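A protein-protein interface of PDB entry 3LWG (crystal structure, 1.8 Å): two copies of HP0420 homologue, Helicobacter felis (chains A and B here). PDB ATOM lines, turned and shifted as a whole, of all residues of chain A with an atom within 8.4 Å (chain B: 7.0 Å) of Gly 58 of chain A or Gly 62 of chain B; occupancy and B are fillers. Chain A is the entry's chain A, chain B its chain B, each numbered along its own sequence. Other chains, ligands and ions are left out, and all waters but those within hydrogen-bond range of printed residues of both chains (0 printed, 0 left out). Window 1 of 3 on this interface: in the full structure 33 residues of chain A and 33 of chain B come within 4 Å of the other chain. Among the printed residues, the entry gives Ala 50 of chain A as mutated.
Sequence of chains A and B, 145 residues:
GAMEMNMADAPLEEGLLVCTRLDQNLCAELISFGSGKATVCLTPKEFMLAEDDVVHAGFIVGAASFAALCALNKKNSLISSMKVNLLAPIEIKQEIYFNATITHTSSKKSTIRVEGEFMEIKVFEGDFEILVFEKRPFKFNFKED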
ATOM      1  N   LEU A  26      -6.911  40.805 -25.491  1.00  0.00           N
ATOM      2  CA  LEU A  26      -5.902  39.755 -25.285  1.00  0.00           C
ATOM      3  C   LEU A  26      -6.313  38.431 -25.940  1.00  0.00           C
ATOM      4  O   LEU A  26      -5.585  37.417 -25.844  1.00  0.00           O
ATOM      5  CB  LEU A  26      -5.682  39.499 -23.784  1.00  0.00           C
ATOM      6  CG  LEU A  26      -5.265  40.671 -22.889  1.00  0.00           C
ATOM      7  CD1 LEU A  26      -4.900  40.133 -21.437  1.00  0.00           C
ATOM      8  CD2 LEU A  26      -4.097  41.446 -23.540  1.00  0.00           C
ATOM      9  N   CYS A  27      -7.495  38.397 -26.535  1.00  0.00           N
ATOM     10  CA  CYS A  27      -7.996  37.127 -27.062  1.00  0.00           C
ATOM     11  C   CYS A  27      -8.317  37.135 -28.603  1.00  0.00           C
ATOM     12  O   CYS A  27      -7.560  36.560 -29.380  1.00  0.00           O
ATOM     13  CB  CYS A  27      -9.191  36.642 -26.232  1.00  0.00           C
ATOM     14  SG  CYS A  27      -9.947  35.092 -26.850  1.00  0.00           S
ATOM     15  N   LEU A  42      -9.121  36.655 -34.769  1.00  0.00           N
ATOM     16  CA  LEU A  42      -7.859  36.875 -34.025  1.00  0.00           C
ATOM     17  C   LEU A  42      -6.974  37.670 -34.979  1.00  0.00           C
ATOM     18  O   LEU A  42      -6.699  37.206 -36.108  1.00  0.00           O
ATOM     19  CB  LEU A  42      -7.188  35.532 -33.706  1.00  0.00           C
ATOM     20  CG  LEU A  42      -5.718  35.531 -33.184  1.00  0.00           C
ATOM     21  CD1 LEU A  42      -5.561  36.327 -31.885  1.00  0.00           C
ATOM     22  CD2 LEU A  42      -5.159  34.112 -32.993  1.00  0.00           C
ATOM     23  N   MET A  48       1.589  38.058 -28.257  1.00  0.00           N
ATOM     24  CA  MET A  48       1.106  36.677 -28.396  1.00  0.00           C
ATOM     25  C   MET A  48       2.151  35.736 -28.991  1.00  0.00           C
ATOM     26  O   MET A  48       1.904  34.544 -29.121  1.00  0.00           O
ATOM     27  CB  MET A  48      -0.153  36.620 -29.252  1.00  0.00           C
ATOM     28  CG  MET A  48      -1.277  37.488 -28.733  1.00  0.00           C
ATOM     29  SD  MET A  48      -2.631  37.330 -29.915  1.00  0.00           S
ATOM     30  CE  MET A  48      -3.937  38.146 -29.011  1.00  0.00           C
ATOM     31  N   ALA A  50       5.191  33.200 -29.544  1.00  0.00           N
ATOM     32  CA  ALA A  50       6.060  32.248 -28.877  1.00  0.00           C
ATOM     33  C   ALA A  50       7.482  32.376 -29.456  1.00  0.00           C
ATOM     34  O   ALA A  50       8.476  32.275 -28.725  1.00  0.00           O
ATOM     35  CB  ALA A  50       5.524  30.824 -29.056  1.00  0.00           C
ATOM     36  N   VAL A  55       2.770  32.338 -33.397  1.00  0.00           N
ATOM     37  CA  VAL A  55       1.950  32.770 -32.293  1.00  0.00           C
ATOM     38  C   VAL A  55       1.847  31.580 -31.319  1.00  0.00           C
ATOM     39  O   VAL A  55       1.684  30.449 -31.727  1.00  0.00           O
ATOM     40  CB  VAL A  55       0.527  33.173 -32.799  1.00  0.00           C
ATOM     41  CG1 VAL A  55      -0.477  33.318 -31.650  1.00  0.00           C
ATOM     42  CG2 VAL A  55       0.596  34.501 -33.604  1.00  0.00           C
ATOM     43  N   HIS A  56       1.881  31.881 -30.033  1.00  0.00           N
ATOM     44  CA  HIS A  56       1.832  30.856 -28.978  1.00  0.00           C
ATOM     45  C   HIS A  56       0.502  30.082 -29.033  1.00  0.00           C
ATOM     46  O   HIS A  56      -0.573  30.687 -29.233  1.00  0.00           O
ATOM     47  CB  HIS A  56       2.027  31.578 -27.641  1.00  0.00           C
ATOM     48  CG  HIS A  56       2.018  30.676 -26.445  1.00  0.00           C
ATOM     49  ND1 HIS A  56       1.155  30.887 -25.393  1.00  0.00           N
ATOM     50  CD2 HIS A  56       2.739  29.585 -26.135  1.00  0.00           C
ATOM     51  CE1 HIS A  56       1.364  29.974 -24.463  1.00  0.00           C
ATOM     52  NE2 HIS A  56       2.305  29.157 -24.892  1.00  0.00           N
ATOM     53  N   ALA A  57       0.580  28.774 -28.820  1.00  0.00           N
ATOM     54  CA  ALA A  57      -0.600  27.899 -28.915  1.00  0.00           C
ATOM     55  C   ALA A  57      -1.708  28.324 -27.940  1.00  0.00           C
ATOM     56  O   ALA A  57      -2.892  28.146 -28.228  1.00  0.00           O
ATOM     57  CB  ALA A  57      -0.232  26.417 -28.689  1.00  0.00           C
ATOM     58  N   GLY A  58      -1.325  28.954 -26.839  1.00  0.00           N
ATOM     59  CA  GLY A  58      -2.332  29.424 -25.895  1.00  0.00           C
ATOM     60  C   GLY A  58      -3.299  30.426 -26.521  1.00  0.00           C
ATOM     61  O   GLY A  58      -4.501  30.416 -26.214  1.00  0.00           O
ATOM     62  N   PHE A  59      -2.794  31.305 -27.384  1.00  0.00           N
ATOM     63  CA  PHE A  59      -3.649  32.325 -27.956  1.00  0.00           C
ATOM     64  C   PHE A  59      -4.447  31.770 -29.126  1.00  0.00           C
ATOM     65  O   PHE A  59      -5.566  32.216 -29.406  1.00  0.00           O
ATOM     66  CB  PHE A  59      -2.875  33.576 -28.381  1.00  0.00           C
ATOM     67  CG  PHE A  59      -2.325  34.335 -27.226  1.00  0.00           C
ATOM     68  CD1 PHE A  59      -3.161  35.176 -26.453  1.00  0.00           C
ATOM     69  CD2 PHE A  59      -0.979  34.164 -26.842  1.00  0.00           C
ATOM     70  CE1 PHE A  59      -2.645  35.887 -25.331  1.00  0.00           C
ATOM     71  CE2 PHE A  59      -0.470  34.839 -25.734  1.00  0.00           C
ATOM     72  CZ  PHE A  59      -1.282  35.706 -24.980  1.00  0.00           C
ATOM     73  N   ILE A  60      -3.888  30.801 -29.808  1.00  0.00           N
ATOM     74  CA  ILE A  60      -4.646  30.207 -30.891  1.00  0.00           C
ATOM     75  C   ILE A  60      -5.818  29.378 -30.307  1.00  0.00           C
ATOM     76  O   ILE A  60      -6.981  29.542 -30.688  1.00  0.00           O
ATOM     77  CB  ILE A  60      -3.743  29.379 -31.799  1.00  0.00           C
ATOM     78  CG1 ILE A  60      -2.746  30.320 -32.520  1.00  0.00           C
ATOM     79  CG2 ILE A  60      -4.599  28.614 -32.839  1.00  0.00           C
ATOM     80  CD1 ILE A  60      -1.581  29.599 -33.019  1.00  0.00           C
ATOM     81  N   VAL A  61      -5.515  28.516 -29.355  1.00  0.00           N
ATOM     82  CA  VAL A  61      -6.572  27.745 -28.670  1.00  0.00           C
ATOM     83  C   VAL A  61      -7.513  28.645 -27.860  1.00  0.00           C
ATOM     84  O   VAL A  61      -8.707  28.368 -27.709  1.00  0.00           O
ATOM     85  CB  VAL A  61      -5.913  26.666 -27.733  1.00  0.00           C
ATOM     86  CG1 VAL A  61      -6.923  26.100 -26.774  1.00  0.00           C
ATOM     87  CG2 VAL A  61      -5.240  25.522 -28.601  1.00  0.00           C
ATOM     88  N   GLY A  62      -6.970  29.726 -27.326  1.00  0.00           N
ATOM     89  CA  GLY A  62      -7.776  30.643 -26.524  1.00  0.00           C
ATOM     90  C   GLY A  62      -8.816  31.319 -27.446  1.00  0.00           C
ATOM     91  O   GLY A  62      -9.945  31.482 -27.053  1.00  0.00           O
ATOM     92  N   ALA A  63      -8.424  31.695 -28.676  1.00  0.00           N
ATOM     93  CA  ALA A  63      -9.395  32.315 -29.582  1.00  0.00           C
ATOM     94  C   ALA A  63     -10.497  31.312 -29.952  1.00  0.00           C
ATOM     95  O   ALA A  63     -11.697  31.626 -30.005  1.00  0.00           O
ATOM     96  CB  ALA A  63      -8.711  32.806 -30.831  1.00  0.00           C
ATOM     97  N   ALA A  64     -10.067  30.094 -30.225  1.00  0.00           N
ATOM     98  CA  ALA A  64     -10.984  29.011 -30.613  1.00  0.00           C
ATOM     99  C   ALA A  64     -11.924  28.744 -29.447  1.00  0.00           C
ATOM    100  O   ALA A  64     -13.094  28.493 -29.641  1.00  0.00           O
ATOM    101  CB  ALA A  64     -10.183  27.736 -30.976  1.00  0.00           C
ATOM    102  N   SER A  65     -11.398  28.772 -28.225  1.00  0.00           N
ATOM    103  CA  SER A  65     -12.234  28.442 -27.074  1.00  0.00           C
ATOM    104  C   SER A  65     -13.320  29.498 -26.869  1.00  0.00           C
ATOM    105  O   SER A  65     -14.458  29.159 -26.459  1.00  0.00           O
ATOM    106  CB  SER A  65     -11.376  28.429 -25.795  1.00  0.00           C
ATOM    107  OG  SER A  65     -10.403  27.403 -25.856  1.00  0.00           O
ATOM    108  N   MET A  82     -10.502  19.166 -25.012  1.00  0.00           N
ATOM    109  CA  MET A  82     -10.408  19.503 -26.424  1.00  0.00           C
ATOM    110  C   MET A  82      -9.476  18.566 -27.150  1.00  0.00           C
ATOM    111  O   MET A  82      -8.554  18.049 -26.555  1.00  0.00           O
ATOM    112  CB  MET A  82      -9.924  20.949 -26.628  1.00  0.00           C
ATOM    113  CG  MET A  82      -8.550  21.280 -26.107  1.00  0.00           C
ATOM    114  SD  MET A  82      -8.214  23.091 -26.158  1.00  0.00           S
ATOM    115  CE  MET A  82      -9.075  23.793 -24.773  1.00  0.00           C
ATOM    116  N   LEU A  86      -3.181  22.008 -34.932  1.00  0.00           N
ATOM    117  CA  LEU A  86      -2.714  23.301 -35.388  1.00  0.00           C
ATOM    118  C   LEU A  86      -2.109  23.009 -36.747  1.00  0.00           C
ATOM    119  O   LEU A  86      -1.093  22.333 -36.836  1.00  0.00           O
ATOM    120  CB  LEU A  86      -1.667  23.856 -34.417  1.00  0.00           C
ATOM    121  CG  LEU A  86      -2.168  23.959 -32.961  1.00  0.00           C
ATOM    122  CD1 LEU A  86      -1.139  24.578 -31.979  1.00  0.00           C
ATOM    123  CD2 LEU A  86      -3.461  24.737 -32.933  1.00  0.00           C
ATOM    124  N   LEU B  22       8.389  34.370 -25.892  1.00  0.00           N
ATOM    125  CA  LEU B  22       7.233  34.187 -24.997  1.00  0.00           C
ATOM    126  C   LEU B  22       7.367  35.009 -23.713  1.00  0.00           C
ATOM    127  O   LEU B  22       8.353  34.872 -22.976  1.00  0.00           O
ATOM    128  CB  LEU B  22       7.032  32.728 -24.670  1.00  0.00           C
ATOM    129  CG  LEU B  22       5.762  32.426 -23.874  1.00  0.00           C
ATOM    130  CD1 LEU B  22       4.505  32.853 -24.606  1.00  0.00           C
ATOM    131  CD2 LEU B  22       5.737  30.904 -23.545  1.00  0.00           C
ATOM    132  N   LEU B  26       2.509  36.467 -19.287  1.00  0.00           N
ATOM    133  CA  LEU B  26       1.197  36.148 -19.937  1.00  0.00           C
ATOM    134  C   LEU B  26       0.970  34.634 -20.012  1.00  0.00           C
ATOM    135  O   LEU B  26      -0.005  34.186 -20.596  1.00  0.00           O
ATOM    136  CB  LEU B  26       1.161  36.680 -21.382  1.00  0.00           C
ATOM    137  CG  LEU B  26       1.083  38.177 -21.676  1.00  0.00           C
ATOM    138  CD1 LEU B  26       1.593  38.533 -23.053  1.00  0.00           C
ATOM    139  CD2 LEU B  26      -0.347  38.545 -21.616  1.00  0.00           C
ATOM    140  N   CYS B  27       1.878  33.854 -19.435  1.00  0.00           N
ATOM    141  CA  CYS B  27       1.826  32.399 -19.600  1.00  0.00           C
ATOM    142  C   CYS B  27       1.998  31.589 -18.284  1.00  0.00           C
ATOM    143  O   CYS B  27       1.036  31.063 -17.716  1.00  0.00           O
ATOM    144  CB  CYS B  27       2.875  31.959 -20.649  1.00  0.00           C
ATOM    145  SG  CYS B  27       2.708  30.170 -21.066  1.00  0.00           S
ATOM    146  N   ALA B  28       3.233  31.403 -17.875  1.00  0.00           N
ATOM    147  CA  ALA B  28       3.583  30.743 -16.618  1.00  0.00           C
ATOM    148  C   ALA B  28       5.068  31.033 -16.360  1.00  0.00           C
ATOM    149  O   ALA B  28       5.838  31.372 -17.268  1.00  0.00           O
ATOM    150  CB  ALA B  28       3.380  29.217 -16.692  1.00  0.00           C
ATOM    151  N   VAL B  40       6.478  24.338 -15.200  1.00  0.00           N
ATOM    152  CA  VAL B  40       6.187  25.766 -15.189  1.00  0.00           C
ATOM    153  C   VAL B  40       5.069  25.950 -14.161  1.00  0.00           C
ATOM    154  O   VAL B  40       4.338  24.978 -13.865  1.00  0.00           O
ATOM    155  CB  VAL B  40       5.732  26.319 -16.625  1.00  0.00           C
ATOM    156  CG1 VAL B  40       6.791  25.969 -17.690  1.00  0.00           C
ATOM    157  CG2 VAL B  40       4.310  25.759 -17.070  1.00  0.00           C
ATOM    158  N   HIS B  56      -9.579  31.388 -18.290  1.00  0.00           N
ATOM    159  CA  HIS B  56      -9.864  31.084 -19.667  1.00  0.00           C
ATOM    160  C   HIS B  56      -8.995  29.916 -20.122  1.00  0.00           C
ATOM    161  O   HIS B  56      -7.794  29.804 -19.726  1.00  0.00           O
ATOM    162  CB  HIS B  56      -9.515  32.301 -20.530  1.00  0.00           C
ATOM    163  CG  HIS B  56      -9.958  32.132 -21.938  1.00  0.00           C
ATOM    164  ND1 HIS B  56      -9.166  32.434 -23.033  1.00  0.00           N
ATOM    165  CD2 HIS B  56     -11.131  31.715 -22.425  1.00  0.00           C
ATOM    166  CE1 HIS B  56      -9.848  32.203 -24.135  1.00  0.00           C
ATOM    167  NE2 HIS B  56     -11.036  31.750 -23.795  1.00  0.00           N
ATOM    168  N   ALA B  57      -9.596  29.015 -20.906  1.00  0.00           N
ATOM    169  CA  ALA B  57      -8.847  27.810 -21.325  1.00  0.00           C
ATOM    170  C   ALA B  57      -7.588  28.143 -22.083  1.00  0.00           C
ATOM    171  O   ALA B  57      -6.644  27.347 -22.078  1.00  0.00           O
ATOM    172  CB  ALA B  57      -9.742  26.831 -22.204  1.00  0.00           C
ATOM    173  N   GLY B  58      -7.539  29.303 -22.726  1.00  0.00           N
ATOM    174  CA  GLY B  58      -6.334  29.639 -23.483  1.00  0.00           C
ATOM    175  C   GLY B  58      -5.124  29.734 -22.544  1.00  0.00           C
ATOM    176  O   GLY B  58      -4.039  29.284 -22.880  1.00  0.00           O
ATOM    177  N   PHE B  59      -5.308  30.286 -21.345  1.00  0.00           N
ATOM    178  CA  PHE B  59      -4.176  30.372 -20.383  1.00  0.00           C
ATOM    179  C   PHE B  59      -3.809  29.019 -19.749  1.00  0.00           C
ATOM    180  O   PHE B  59      -2.615  28.731 -19.523  1.00  0.00           O
ATOM    181  CB  PHE B  59      -4.408  31.500 -19.324  1.00  0.00           C
ATOM    182  CG  PHE B  59      -4.454  32.829 -19.945  1.00  0.00           C
ATOM    183  CD1 PHE B  59      -3.268  33.433 -20.400  1.00  0.00           C
ATOM    184  CD2 PHE B  59      -5.678  33.470 -20.188  1.00  0.00           C
ATOM    185  CE1 PHE B  59      -3.323  34.642 -21.063  1.00  0.00           C
ATOM    186  CE2 PHE B  59      -5.695  34.716 -20.847  1.00  0.00           C
ATOM    187  CZ  PHE B  59      -4.541  35.280 -21.257  1.00  0.00           C
ATOM    188  N   ILE B  60      -4.802  28.163 -19.512  1.00  0.00           N
ATOM    189  CA  ILE B  60      -4.503  26.818 -18.955  1.00  0.00           C
ATOM    190  C   ILE B  60      -3.728  25.990 -19.997  1.00  0.00           C
ATOM    191  O   ILE B  60      -2.648  25.437 -19.749  1.00  0.00           O
ATOM    192  CB  ILE B  60      -5.812  26.104 -18.592  1.00  0.00           C
ATOM    193  CG1 ILE B  60      -6.601  26.956 -17.556  1.00  0.00           C
ATOM    194  CG2 ILE B  60      -5.600  24.672 -18.058  1.00  0.00           C
ATOM    195  CD1 ILE B  60      -5.840  27.166 -16.290  1.00  0.00           C
ATOM    196  N   VAL B  61      -4.308  25.889 -21.188  1.00  0.00           N
ATOM    197  CA  VAL B  61      -3.611  25.190 -22.260  1.00  0.00           C
ATOM    198  C   VAL B  61      -2.286  25.872 -22.672  1.00  0.00           C
ATOM    199  O   VAL B  61      -1.286  25.185 -22.980  1.00  0.00           O
ATOM    200  CB  VAL B  61      -4.572  24.961 -23.444  1.00  0.00           C
ATOM    201  CG1 VAL B  61      -3.800  24.441 -24.654  1.00  0.00           C
ATOM    202  CG2 VAL B  61      -5.651  23.969 -23.026  1.00  0.00           C
ATOM    203  N   GLY B  62      -2.252  27.196 -22.670  1.00  0.00           N
ATOM    204  CA  GLY B  62      -1.036  27.928 -22.971  1.00  0.00           C
ATOM    205  C   GLY B  62       0.122  27.590 -22.034  1.00  0.00           C
ATOM    206  O   GLY B  62       1.257  27.384 -22.497  1.00  0.00           O
ATOM    207  N   ALA B  63      -0.175  27.528 -20.734  1.00  0.00           N
ATOM    208  CA  ALA B  63       0.842  27.155 -19.726  1.00  0.00           C
ATOM    209  C   ALA B  63       1.343  25.737 -19.980  1.00  0.00           C
ATOM    210  O   ALA B  63       2.547  25.477 -19.975  1.00  0.00           O
ATOM    211  CB  ALA B  63       0.235  27.286 -18.317  1.00  0.00           C
ATOM    212  N   ALA B  64       0.418  24.813 -20.245  1.00  0.00           N
ATOM    213  CA  ALA B  64       0.800  23.422 -20.521  1.00  0.00           C
ATOM    214  C   ALA B  64       1.645  23.364 -21.814  1.00  0.00           C
ATOM    215  O   ALA B  64       2.615  22.607 -21.917  1.00  0.00           O
ATOM    216  CB  ALA B  64      -0.449  22.543 -20.649  1.00  0.00           C
ATOM    217  N   SER B  65       1.278  24.165 -22.807  1.00  0.00           N
ATOM    218  CA  SER B  65       2.004  24.174 -24.098  1.00  0.00           C
ATOM    219  C   SER B  65       3.442  24.601 -23.900  1.00  0.00           C
ATOM    220  O   SER B  65       4.390  24.037 -24.496  1.00  0.00           O
ATOM    221  CB  SER B  65       1.353  25.157 -25.115  1.00  0.00           C
ATOM    222  OG  SER B  65       0.042  24.763 -25.430  1.00  0.00           O
ATOM    223  N   PHE B  66       3.607  25.639 -23.090  1.00  0.00           N
ATOM    224  CA  PHE B  66       4.971  26.134 -22.761  1.00  0.00           C
ATOM    225  C   PHE B  66       5.789  25.003 -22.065  1.00  0.00           C
ATOM    226  O   PHE B  66       6.888  24.690 -22.491  1.00  0.00           O
ATOM    227  CB  PHE B  66       4.809  27.345 -21.852  1.00  0.00           C
ATOM    228  CG  PHE B  66       6.093  27.986 -21.384  1.00  0.00           C
ATOM    229  CD1 PHE B  66       7.235  28.033 -22.187  1.00  0.00           C
ATOM    230  CD2 PHE B  66       6.098  28.622 -20.166  1.00  0.00           C
ATOM    231  CE1 PHE B  66       8.402  28.715 -21.714  1.00  0.00           C
ATOM    232  CE2 PHE B  66       7.216  29.315 -19.687  1.00  0.00           C
ATOM    233  CZ  PHE B  66       8.369  29.344 -20.456  1.00  0.00           C
ATOM    234  N   ALA B  67       5.240  24.373 -21.012  1.00  0.00           N
ATOM    235  CA  ALA B  67       5.970  23.256 -20.380  1.00  0.00           C
ATOM    236  C   ALA B  67       6.335  22.190 -21.437  1.00  0.00           C
ATOM    237  O   ALA B  67       7.434  21.662 -21.427  1.00  0.00           O
ATOM    238  CB  ALA B  67       5.130  22.621 -19.257  1.00  0.00           C
ATOM    239  N   ALA B  68       5.395  21.870 -22.335  1.00  0.00           N
ATOM    240  CA  ALA B  68       5.626  20.741 -23.271  1.00  0.00           C
ATOM    241  C   ALA B  68       6.823  21.106 -24.179  1.00  0.00           C
ATOM    242  O   ALA B  68       7.768  20.336 -24.369  1.00  0.00           O
ATOM    243  CB  ALA B  68       4.382  20.456 -24.100  1.00  0.00           C
ATOM    244  N   MET B  82      -2.911  18.546 -30.003  1.00  0.00           N
ATOM    245  CA  MET B  82      -3.012  18.220 -28.592  1.00  0.00           C
ATOM    246  C   MET B  82      -4.364  17.569 -28.280  1.00  0.00           C
ATOM    247  O   MET B  82      -5.379  17.801 -28.991  1.00  0.00           O
ATOM    248  CB  MET B  82      -2.793  19.473 -27.729  1.00  0.00           C
ATOM    249  CG  MET B  82      -3.971  20.463 -27.828  1.00  0.00           C
ATOM    250  SD  MET B  82      -3.620  22.123 -27.202  1.00  0.00           S
ATOM    251  CE  MET B  82      -2.320  22.709 -28.275  1.00  0.00           C
ATOM    252  N   PHE B  98       2.556  22.822 -13.857  1.00  0.00           N
ATOM    253  CA  PHE B  98       2.420  21.933 -15.018  1.00  0.00           C
ATOM    254  C   PHE B  98       3.752  21.194 -15.227  1.00  0.00           C
ATOM    255  O   PHE B  98       4.802  21.832 -15.467  1.00  0.00           O
ATOM    256  CB  PHE B  98       2.123  22.752 -16.277  1.00  0.00           C
ATOM    257  CG  PHE B  98       0.749  23.390 -16.268  1.00  0.00           C
ATOM    258  CD1 PHE B  98      -0.323  22.749 -16.906  1.00  0.00           C
ATOM    259  CD2 PHE B  98       0.535  24.599 -15.590  1.00  0.00           C
ATOM    260  CE1 PHE B  98      -1.660  23.342 -16.888  1.00  0.00           C
ATOM    261  CE2 PHE B  98      -0.750  25.227 -15.580  1.00  0.00           C
ATOM    262  CZ  PHE B  98      -1.860  24.596 -16.215  1.00  0.00           C
ATOM    263  N   PHE B 128       0.648  16.428 -25.941  1.00  0.00           N
ATOM    264  CA  PHE B 128       0.983  17.392 -27.001  1.00  0.00           C
ATOM    265  C   PHE B 128       1.893  16.726 -28.026  1.00  0.00           C
ATOM    266  O   PHE B 128       2.826  16.049 -27.645  1.00  0.00           O
ATOM    267  CB  PHE B 128       1.706  18.578 -26.400  1.00  0.00           C
ATOM    268  CG  PHE B 128       0.829  19.365 -25.474  1.00  0.00           C
ATOM    269  CD1 PHE B 128       0.272  20.548 -25.892  1.00  0.00           C
ATOM    270  CD2 PHE B 128       0.526  18.889 -24.214  1.00  0.00           C
ATOM    271  CE1 PHE B 128      -0.537  21.269 -25.072  1.00  0.00           C
ATOM    272  CE2 PHE B 128      -0.324  19.613 -23.353  1.00  0.00           C
ATOM    273  CZ  PHE B 128      -0.849  20.804 -23.783  1.00  0.00           C
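Cys 27 of chain A touches His 56 of chain B, and with the chains exchanged His 56 of chain A touches Cys 27 of chain B.
Ala 57 of chain A touches Ser 65 of chain B, and with the chains exchanged Ser 65 of chain A touches Ala 57 of chain B.
Gly 58 of chain B touches its own counterpart, Gly 58 of chain A.
Gly 58 of chain A touches Gly 62 of chain B, and with the chains exchanged Gly 62 of chain A touches Gly 58 of chain B.
Of the 13 pairs that touch across the chains among the printed residues, 9 have their exchanged pair printed and touching as well.
NE2 of His 56 of chain A is in hydrogen-bond range of O of Gly 62 of chain B.
A ring nitrogen (NE2) of His 56 of chain B sits close to the backbone carbonyl oxygen of Gly 62 of chain A (3.4 Å).
The side-chain sulfur (SG) of Cys 27 of chain A is in hydrogen-bond range of the backbone carbonyl oxygen (O) of Gly 62 of chain A.
The backbone NH of His 56 of chain A is in hydrogen-bond range of the backbone carbonyl oxygen of Met 48 of chain A, 2.8 Å away.
The backbone NH (N) of Gly 58 of chain A sits close to a ring nitrogen (ND1) of His 56 of chain A, at 3.5 Å.
O of Val 61 of chain A sits at hydrogen-bond distance from OG of Ser 65 of chain A, at 2.7 Å.
O of Gly 62 of chain B is in hydrogen-bond range of SG of Cys 27 of chain B, at 3.5 Å.
The backbone carbonyl oxygen (O) of Val 61 of chain B is in hydrogen-bond range of the side-chain hydroxyl (OG) of Ser 65 of chain B, 2.8 Å away.
Among the printed residues, merely in contact across the chains: Gly 58 of chain A with Gly 58 of chain B, Gly 62 of chain A with Gly 58 of chain B, Ala 50 of chain A with Leu 22 of chain B, Gly 58 of chain A with Gly 62 of chain B, His 56 of chain A with Cys 27 of chain B, Ala 57 of chain A with Ser 65 of chain B, Ser 65 of chain A with Ala 57 of chain B, His 56 of chain A with Leu 22 of chain B, Met 82 of chain A with Val 61 of chain B, Ser 65 of chain A with His 56 of chain B and Cys 27 of chain A with His 56 of chain B.
Gly 62 of chain B touches just these residues of chain A: His 56 and Gly 58.
Printed residues of chain B within 4 Å of Ala 57 of chain A: Ser 65 (3.7 Å).
Of the printed residues of chain A, Leu 22 of chain B touches Ala 50 and His 56.
Ala 67 of chain B touches none of the printed residues of chain A.
The nearest residue of chain A that does not touch Gly 62 of chain B is Ala 57 of chain A (5.0 Å).
The nearest printed residue of chain A that does not touch Gly 58 of chain B is Val 61 of chain A (4.6 Å).
Of the 18 printed residues of chain A, 8 touch a printed residue of chain B.
Hydrophobic or aromatic side chains of chain A that line the printed part of chain B: His 56, Ala 57 and Met 82.
Of the 21 printed residues of chain B, 8 touch a printed residue of chain A.
Hydrophobic or aromatic side chains of chain B within 4 Å of the printed part of chain A: Leu 22, His 56, Ala 57 and Val 61.
Among the printed residues, 13 pairs touch across the chains.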
